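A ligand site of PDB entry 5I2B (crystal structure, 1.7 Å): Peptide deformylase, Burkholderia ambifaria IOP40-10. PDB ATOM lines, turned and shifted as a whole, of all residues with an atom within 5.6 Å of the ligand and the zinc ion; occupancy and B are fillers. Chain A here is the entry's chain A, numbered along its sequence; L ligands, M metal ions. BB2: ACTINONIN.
The zinc ion is bound by a ring nitrogen (NE2) of His 149, an oxygen (O4) of the ligand, a ring nitrogen (NE2) of His 153, the side-chain sulfur (SG) of Cys 107 and an oxygen (O2) of the ligand.
The side-chain carboxylate (OE1) of Glu 105 sits at hydrogen-bond distance from a ring nitrogen (ND1) of His 149, at 2.8 Å. The backbone NH of Ser 109 sits close to the side-chain sulfur of Cys 107 (3.4 Å). OE1 of Glu 150 lies within hydrogen-bond range of N of Ala 56. The side-chain amide oxygen (OE1) of Gln 59 lies within hydrogen-bond range of the backbone NH (N) of Ala 56 (2.9 Å). The side-chain amide nitrogen (NE2) of Gln 59 lies within hydrogen-bond range of the side-chain hydroxyl (OG) of Ser 109, 3.1 Å away. OH of Tyr 77 sits at hydrogen-bond distance from O of Trp 104. OE2 of Glu 105 lies within salt-bridge range of NH1 of Arg 145 (2.8 Å).
A nitrogen (N1) of the ligand lies within hydrogen-bond range of the side-chain carboxylate (OE2) of Glu 150, 2.5 Å away. An oxygen (O2) of the ligand lies close to the side-chain amide oxygen (OE1) of Gln 59 (2.7 Å). N of Ala 53 lies within hydrogen-bond range of O13 of the ligand (2.7 Å). The backbone NH of Leu 108 lies close to an oxygen (O4) of the ligand (2.8 Å). O20 of the ligand sits at hydrogen-bond distance from N of Gly 106 (2.8 Å). A nitrogen (N14) of the ligand lies within hydrogen-bond range of the backbone carbonyl oxygen (O) of Gly 106 (3.2 Å). The backbone carbonyl oxygen of Gly 54 sits at hydrogen-bond distance from a nitrogen (N1) of the ligand (3.1 Å). An oxygen (O27) of the ligand sits at hydrogen-bond distance from the backbone carbonyl oxygen of Trp 104, 3.3 Å away.
Merely in contact with the zinc ion: Gln 59. Of the 23 residues printed, 4 come within 4 Å of the zinc ion.
Asn 51 touches the ligand (O to C18, 3.8 Å). Gly 52 touches the ligand. C of Glu 105 touches O20 of the ligand, at 3.7 Å. Arg 114 touches the ligand. Phe 142 touches the ligand (CE1 to C11, 3.5 Å). Of the 23 residues printed, 15 come within 4 Å of the ligand. Along chain A the residues within 4 Å of the ligand span positions 51 to 153. The nearest printed residue that does not touch the ligand is Arg 145 (4.004 Å).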
ATOM      1  N   ALA A  50     -15.928  30.759   9.905  1.00  0.00           N
ATOM      2  CA  ALA A  50     -15.137  29.600   9.512  1.00  0.00           C
ATOM      3  C   ALA A  50     -14.169  29.152  10.593  1.00  0.00           C
ATOM      4  O   ALA A  50     -13.371  28.229  10.354  1.00  0.00           O
ATOM      5  CB  ALA A  50     -14.369  29.909   8.221  1.00  0.00           C
ATOM      6  N   ASN A  51     -14.207  29.774  11.772  1.00  0.00           N
ATOM      7  CA  ASN A  51     -13.319  29.430  12.888  1.00  0.00           C
ATOM      8  C   ASN A  51     -11.851  29.578  12.512  1.00  0.00           C
ATOM      9  O   ASN A  51     -10.994  28.779  12.922  1.00  0.00           O
ATOM     10  CB  ASN A  51     -13.626  28.020  13.409  1.00  0.00           C
ATOM     11  CG  ASN A  51     -15.054  27.880  13.885  1.00  0.00           C
ATOM     12  OD1 ASN A  51     -15.471  28.549  14.830  1.00  0.00           O
ATOM     13  ND2 ASN A  51     -15.816  27.014  13.227  1.00  0.00           N
ATOM     14  N   GLY A  52     -11.541  30.624  11.739  1.00  0.00           N
ATOM     15  CA  GLY A  52     -10.183  30.878  11.316  1.00  0.00           C
ATOM     16  C   GLY A  52      -9.387  31.698  12.328  1.00  0.00           C
ATOM     17  O   GLY A  52      -9.935  32.434  13.147  1.00  0.00           O
ATOM     18  N   ALA A  53      -8.060  31.528  12.262  1.00  0.00           N
ATOM     19  CA  ALA A  53      -7.157  32.322  13.081  1.00  0.00           C
ATOM     20  C   ALA A  53      -6.743  33.624  12.405  1.00  0.00           C
ATOM     21  O   ALA A  53      -6.208  34.509  13.077  1.00  0.00           O
ATOM     22  CB  ALA A  53      -5.892  31.516  13.410  1.00  0.00           C
ATOM     23  N   GLY A  54      -6.976  33.743  11.089  1.00  0.00           N
ATOM     24  CA  GLY A  54      -6.709  34.956  10.336  1.00  0.00           C
ATOM     25  C   GLY A  54      -7.416  34.897   8.997  1.00  0.00           C
ATOM     26  O   GLY A  54      -7.962  33.865   8.596  1.00  0.00           O
ATOM     27  N   LEU A  55      -7.437  36.050   8.308  1.00  0.00           N
ATOM     28  CA  LEU A  55      -8.031  36.156   6.986  1.00  0.00           C
ATOM     29  C   LEU A  55      -7.371  37.323   6.246  1.00  0.00           C
ATOM     30  O   LEU A  55      -6.966  38.305   6.869  1.00  0.00           O
ATOM     31  CB  LEU A  55      -9.550  36.373   7.063  1.00  0.00           C
ATOM     32  CG  LEU A  55     -10.324  36.182   5.745  1.00  0.00           C
ATOM     33  CD1 LEU A  55     -10.431  34.692   5.416  1.00  0.00           C
ATOM     34  CD2 LEU A  55     -11.716  36.781   5.827  1.00  0.00           C
ATOM     35  N   ALA A  56      -7.255  37.201   4.931  1.00  0.00           N
ATOM     36  CA  ALA A  56      -6.703  38.248   4.088  1.00  0.00           C
ATOM     37  C   ALA A  56      -7.759  38.708   3.088  1.00  0.00           C
ATOM     38  O   ALA A  56      -8.535  37.888   2.594  1.00  0.00           O
ATOM     39  CB  ALA A  56      -5.436  37.751   3.366  1.00  0.00           C
ATOM     40  N   GLN A  59      -8.869  36.893  -0.087  1.00  0.00           N
ATOM     41  CA  GLN A  59      -9.659  35.688   0.074  1.00  0.00           C
ATOM     42  C   GLN A  59     -11.156  35.952  -0.047  1.00  0.00           C
ATOM     43  O   GLN A  59     -11.908  35.008  -0.329  1.00  0.00           O
ATOM     44  CB  GLN A  59      -9.366  35.043   1.428  1.00  0.00           C
ATOM     45  CG  GLN A  59      -7.980  34.437   1.559  1.00  0.00           C
ATOM     46  CD  GLN A  59      -7.803  33.792   2.900  1.00  0.00           C
ATOM     47  OE1 GLN A  59      -7.470  34.463   3.869  1.00  0.00           O
ATOM     48  NE2 GLN A  59      -8.069  32.492   2.974  1.00  0.00           N
ATOM     49  N   ARG A  76      -2.083  22.121  18.698  1.00  0.00           N
ATOM     50  CA  ARG A  76      -0.879  21.940  17.911  1.00  0.00           C
ATOM     51  C   ARG A  76       0.200  22.935  18.310  1.00  0.00           C
ATOM     52  O   ARG A  76       1.401  22.660  18.108  1.00  0.00           O
ATOM     53  CB  ARG A  76      -1.194  22.067  16.415  1.00  0.00           C
ATOM     54  N   TYR A  77      -0.193  24.062  18.888  1.00  0.00           N
ATOM     55  CA  TYR A  77       0.720  25.079  19.391  1.00  0.00           C
ATOM     56  C   TYR A  77       0.274  25.454  20.803  1.00  0.00           C
ATOM     57  O   TYR A  77      -0.212  26.568  21.038  1.00  0.00           O
ATOM     58  CB  TYR A  77       0.751  26.288  18.460  1.00  0.00           C
ATOM     59  CG  TYR A  77       0.995  25.904  17.018  1.00  0.00           C
ATOM     60  CD1 TYR A  77      -0.055  25.516  16.197  1.00  0.00           C
ATOM     61  CD2 TYR A  77       2.278  25.908  16.492  1.00  0.00           C
ATOM     62  CE1 TYR A  77       0.170  25.152  14.872  1.00  0.00           C
ATOM     63  CE2 TYR A  77       2.504  25.538  15.174  1.00  0.00           C
ATOM     64  CZ  TYR A  77       1.446  25.163  14.369  1.00  0.00           C
ATOM     65  OH  TYR A  77       1.673  24.809  13.064  1.00  0.00           O
ATOM     66  N   TRP A 104       2.013  22.233  10.960  1.00  0.00           N
ATOM     67  CA  TRP A 104       0.838  21.980  10.135  1.00  0.00           C
ATOM     68  C   TRP A 104       0.040  23.257   9.914  1.00  0.00           C
ATOM     69  O   TRP A 104      -0.200  24.027  10.842  1.00  0.00           O
ATOM     70  CB  TRP A 104      -0.056  20.947  10.798  1.00  0.00           C
ATOM     71  CG  TRP A 104       0.539  19.589  10.793  1.00  0.00           C
ATOM     72  CD1 TRP A 104       1.191  18.966  11.812  1.00  0.00           C
ATOM     73  CD2 TRP A 104       0.520  18.661   9.702  1.00  0.00           C
ATOM     74  NE1 TRP A 104       1.586  17.703  11.430  1.00  0.00           N
ATOM     75  CE2 TRP A 104       1.180  17.499  10.134  1.00  0.00           C
ATOM     76  CE3 TRP A 104       0.014  18.705   8.406  1.00  0.00           C
ATOM     77  CZ2 TRP A 104       1.352  16.386   9.308  1.00  0.00           C
ATOM     78  CZ3 TRP A 104       0.176  17.599   7.589  1.00  0.00           C
ATOM     79  CH2 TRP A 104       0.839  16.453   8.047  1.00  0.00           C
ATOM     80  N   GLU A 105      -0.377  23.465   8.669  1.00  0.00           N
ATOM     81  CA  GLU A 105      -1.232  24.584   8.310  1.00  0.00           C
ATOM     82  C   GLU A 105      -2.423  24.099   7.485  1.00  0.00           C
ATOM     83  O   GLU A 105      -2.315  23.146   6.721  1.00  0.00           O
ATOM     84  CB  GLU A 105      -0.490  25.645   7.493  1.00  0.00           C
ATOM     85  CG  GLU A 105       0.721  26.198   8.220  1.00  0.00           C
ATOM     86  CD  GLU A 105       1.324  27.417   7.543  1.00  0.00           C
ATOM     87  OE1 GLU A 105       0.711  28.005   6.629  1.00  0.00           O
ATOM     88  OE2 GLU A 105       2.422  27.814   7.976  1.00  0.00           O
ATOM     89  N   GLY A 106      -3.547  24.781   7.664  1.00  0.00           N
ATOM     90  CA  GLY A 106      -4.637  24.694   6.732  1.00  0.00           C
ATOM     91  C   GLY A 106      -5.034  26.104   6.307  1.00  0.00           C
ATOM     92  O   GLY A 106      -4.635  27.077   6.939  1.00  0.00           O
ATOM     93  N   CYS A 107      -5.843  26.179   5.264  1.00  0.00           N
ATOM     94  CA  CYS A 107      -6.241  27.463   4.694  1.00  0.00           C
ATOM     95  C   CYS A 107      -7.711  27.395   4.314  1.00  0.00           C
ATOM     96  O   CYS A 107      -8.150  26.411   3.728  1.00  0.00           O
ATOM     97  CB  CYS A 107      -5.404  27.788   3.446  1.00  0.00           C
ATOM     98  SG  CYS A 107      -5.746  29.426   2.775  1.00  0.00           S
ATOM     99  N   LEU A 108      -8.462  28.461   4.630  1.00  0.00           N
ATOM    100  CA  LEU A 108      -9.859  28.464   4.257  1.00  0.00           C
ATOM    101  C   LEU A 108     -10.051  28.438   2.738  1.00  0.00           C
ATOM    102  O   LEU A 108     -11.119  28.043   2.256  1.00  0.00           O
ATOM    103  CB  LEU A 108     -10.559  29.676   4.865  1.00  0.00           C
ATOM    104  CG  LEU A 108     -10.588  29.615   6.401  1.00  0.00           C
ATOM    105  CD1 LEU A 108     -11.242  30.880   6.929  1.00  0.00           C
ATOM    106  CD2 LEU A 108     -11.354  28.367   6.881  1.00  0.00           C
ATOM    107  N   SER A 109      -9.042  28.872   1.980  1.00  0.00           N
ATOM    108  CA  SER A 109      -9.087  28.783   0.520  1.00  0.00           C
ATOM    109  C   SER A 109      -8.645  27.416  -0.006  1.00  0.00           C
ATOM    110  O   SER A 109      -8.716  27.183  -1.213  1.00  0.00           O
ATOM    111  CB  SER A 109      -8.201  29.876  -0.091  1.00  0.00           C
ATOM    112  OG  SER A 109      -8.691  31.178   0.262  1.00  0.00           O
ATOM    113  N   ARG A 114      -4.505  19.734   4.896  1.00  0.00           N
ATOM    114  CA  ARG A 114      -3.426  20.238   5.749  1.00  0.00           C
ATOM    115  C   ARG A 114      -2.088  19.925   5.102  1.00  0.00           C
ATOM    116  O   ARG A 114      -1.946  18.930   4.371  1.00  0.00           O
ATOM    117  CB  ARG A 114      -3.425  19.610   7.152  1.00  0.00           C
ATOM    118  CG  ARG A 114      -4.683  19.849   7.966  1.00  0.00           C
ATOM    119  CD  ARG A 114      -4.790  21.316   8.391  1.00  0.00           C
ATOM    120  NE  ARG A 114      -5.918  21.521   9.305  1.00  0.00           N
ATOM    121  CZ  ARG A 114      -7.142  21.855   8.918  1.00  0.00           C
ATOM    122  NH1 ARG A 114      -7.427  22.009   7.624  1.00  0.00           N
ATOM    123  NH2 ARG A 114      -8.100  22.015   9.818  1.00  0.00           N
ATOM    124  N   PHE A 142       3.481  30.481  16.812  1.00  0.00           N
ATOM    125  CA  PHE A 142       2.224  30.465  16.064  1.00  0.00           C
ATOM    126  C   PHE A 142       1.824  31.866  15.620  1.00  0.00           C
ATOM    127  O   PHE A 142       1.334  32.056  14.507  1.00  0.00           O
ATOM    128  CB  PHE A 142       1.109  29.831  16.909  1.00  0.00           C
ATOM    129  CG  PHE A 142      -0.186  29.642  16.152  1.00  0.00           C
ATOM    130  CD1 PHE A 142      -0.280  28.707  15.135  1.00  0.00           C
ATOM    131  CD2 PHE A 142      -1.318  30.384  16.478  1.00  0.00           C
ATOM    132  CE1 PHE A 142      -1.469  28.527  14.443  1.00  0.00           C
ATOM    133  CE2 PHE A 142      -2.498  30.214  15.790  1.00  0.00           C
ATOM    134  CZ  PHE A 142      -2.583  29.280  14.772  1.00  0.00           C
ATOM    135  N   ARG A 145       3.675  32.608  12.628  1.00  0.00           N
ATOM    136  CA  ARG A 145       3.203  31.739  11.542  1.00  0.00           C
ATOM    137  C   ARG A 145       1.915  32.274  10.914  1.00  0.00           C
ATOM    138  O   ARG A 145       1.776  32.307   9.683  1.00  0.00           O
ATOM    139  CB  ARG A 145       2.993  30.318  12.075  1.00  0.00           C
ATOM    140  CG  ARG A 145       2.304  29.359  11.071  1.00  0.00           C
ATOM    141  CD  ARG A 145       2.302  27.911  11.536  1.00  0.00           C
ATOM    142  NE  ARG A 145       3.643  27.437  11.886  1.00  0.00           N
ATOM    143  CZ  ARG A 145       4.463  26.797  11.052  1.00  0.00           C
ATOM    144  NH1 ARG A 145       4.061  26.502   9.802  1.00  0.00           N
ATOM    145  NH2 ARG A 145       5.654  26.403  11.481  1.00  0.00           N
ATOM    146  N   VAL A 146       0.973  32.706  11.751  1.00  0.00           N
ATOM    147  CA  VAL A 146      -0.276  33.247  11.209  1.00  0.00           C
ATOM    148  C   VAL A 146      -0.002  34.483  10.364  1.00  0.00           C
ATOM    149  O   VAL A 146      -0.556  34.656   9.274  1.00  0.00           O
ATOM    150  CB  VAL A 146      -1.279  33.554  12.341  1.00  0.00           C
ATOM    151  CG1 VAL A 146      -2.474  34.318  11.777  1.00  0.00           C
ATOM    152  CG2 VAL A 146      -1.724  32.261  13.022  1.00  0.00           C
ATOM    153  N   HIS A 149       1.522  33.431   7.042  1.00  0.00           N
ATOM    154  CA  HIS A 149       0.481  32.842   6.213  1.00  0.00           C
ATOM    155  C   HIS A 149      -0.431  33.911   5.603  1.00  0.00           C
ATOM    156  O   HIS A 149      -0.729  33.883   4.403  1.00  0.00           O
ATOM    157  CB  HIS A 149      -0.309  31.846   7.047  1.00  0.00           C
ATOM    158  CG  HIS A 149      -1.411  31.174   6.305  1.00  0.00           C
ATOM    159  ND1 HIS A 149      -1.381  29.824   5.991  1.00  0.00           N
ATOM    160  CD2 HIS A 149      -2.611  31.646   5.891  1.00  0.00           C
ATOM    161  CE1 HIS A 149      -2.512  29.516   5.374  1.00  0.00           C
ATOM    162  NE2 HIS A 149      -3.278  30.593   5.300  1.00  0.00           N
ATOM    163  N   GLU A 150      -0.874  34.888   6.411  1.00  0.00           N
ATOM    164  CA  GLU A 150      -1.768  35.906   5.846  1.00  0.00           C
ATOM    165  C   GLU A 150      -1.010  36.838   4.916  1.00  0.00           C
ATOM    166  O   GLU A 150      -1.550  37.264   3.882  1.00  0.00           O
ATOM    167  CB  GLU A 150      -2.441  36.716   6.958  1.00  0.00           C
ATOM    168  CG  GLU A 150      -3.198  35.860   7.951  1.00  0.00           C
ATOM    169  CD  GLU A 150      -4.238  34.967   7.286  1.00  0.00           C
ATOM    170  OE1 GLU A 150      -4.705  35.269   6.164  1.00  0.00           O
ATOM    171  OE2 GLU A 150      -4.603  33.966   7.927  1.00  0.00           O
ATOM    172  N   HIS A 153      -0.835  35.617   1.411  1.00  0.00           N
ATOM    173  CA  HIS A 153      -2.033  35.867   0.608  1.00  0.00           C
ATOM    174  C   HIS A 153      -1.950  37.199  -0.143  1.00  0.00           C
ATOM    175  O   HIS A 153      -2.520  37.341  -1.227  1.00  0.00           O
ATOM    176  CB  HIS A 153      -3.293  35.872   1.484  1.00  0.00           C
ATOM    177  CG  HIS A 153      -3.840  34.512   1.794  1.00  0.00           C
ATOM    178  ND1 HIS A 153      -4.244  33.627   0.820  1.00  0.00           N
ATOM    179  CD2 HIS A 153      -4.063  33.887   2.982  1.00  0.00           C
ATOM    180  CE1 HIS A 153      -4.670  32.509   1.384  1.00  0.00           C
ATOM    181  NE2 HIS A 153      -4.582  32.653   2.700  1.00  0.00           N
HETATM  182  C5  BB2 L   1      -6.979  30.635   7.973  1.00  0.00           C
HETATM  183  C3  BB2 L   1      -6.627  31.175   6.603  1.00  0.00           C
HETATM  184  O4  BB2 L   1      -6.818  30.525   5.588  1.00  0.00           O
HETATM  185  N1  BB2 L   1      -6.124  32.400   6.613  1.00  0.00           N
HETATM  186  O2  BB2 L   1      -5.775  32.981   5.398  1.00  0.00           O
HETATM  187  C6  BB2 L   1      -5.781  29.937   8.644  1.00  0.00           C
HETATM  188  C12 BB2 L   1      -6.270  29.096   9.786  1.00  0.00           C
HETATM  189  O13 BB2 L   1      -6.886  29.586  10.733  1.00  0.00           O
HETATM  190  C7  BB2 L   1      -4.830  30.986   9.201  1.00  0.00           C
HETATM  191  C8  BB2 L   1      -3.627  30.431   9.950  1.00  0.00           C
HETATM  192  C9  BB2 L   1      -2.805  29.469   9.130  1.00  0.00           C
HETATM  193  C10 BB2 L   1      -1.486  29.127   9.760  1.00  0.00           C
HETATM  194  C11 BB2 L   1      -1.645  28.194  10.925  1.00  0.00           C
HETATM  195  N14 BB2 L   1      -5.957  27.799   9.714  1.00  0.00           N
HETATM  196  C15 BB2 L   1      -6.317  26.873  10.766  1.00  0.00           C
HETATM  197  C16 BB2 L   1      -7.518  25.987  10.365  1.00  0.00           C
HETATM  198  C18 BB2 L   1      -8.831  26.724  10.575  1.00  0.00           C
HETATM  199  C17 BB2 L   1      -7.411  25.494   8.933  1.00  0.00           C
HETATM  200  C19 BB2 L   1      -5.104  25.993  11.092  1.00  0.00           C
HETATM  201  O20 BB2 L   1      -4.281  25.754  10.228  1.00  0.00           O
HETATM  202  N21 BB2 L   1      -4.975  25.535  12.350  1.00  0.00           N
HETATM  203  C22 BB2 L   1      -3.848  24.657  12.707  1.00  0.00           C
HETATM  204  C23 BB2 L   1      -5.881  25.816  13.480  1.00  0.00           C
HETATM  205  C24 BB2 L   1      -5.170  25.261  14.682  1.00  0.00           C
HETATM  206  C25 BB2 L   1      -3.908  24.590  14.236  1.00  0.00           C
HETATM  207  C26 BB2 L   1      -3.967  23.297  12.033  1.00  0.00           C
HETATM  208  O27 BB2 L   1      -2.772  22.559  12.187  1.00  0.00           O
HETATM  209 ZN    ZN M   1      -5.105  31.059   4.236  1.00  0.00          ZN
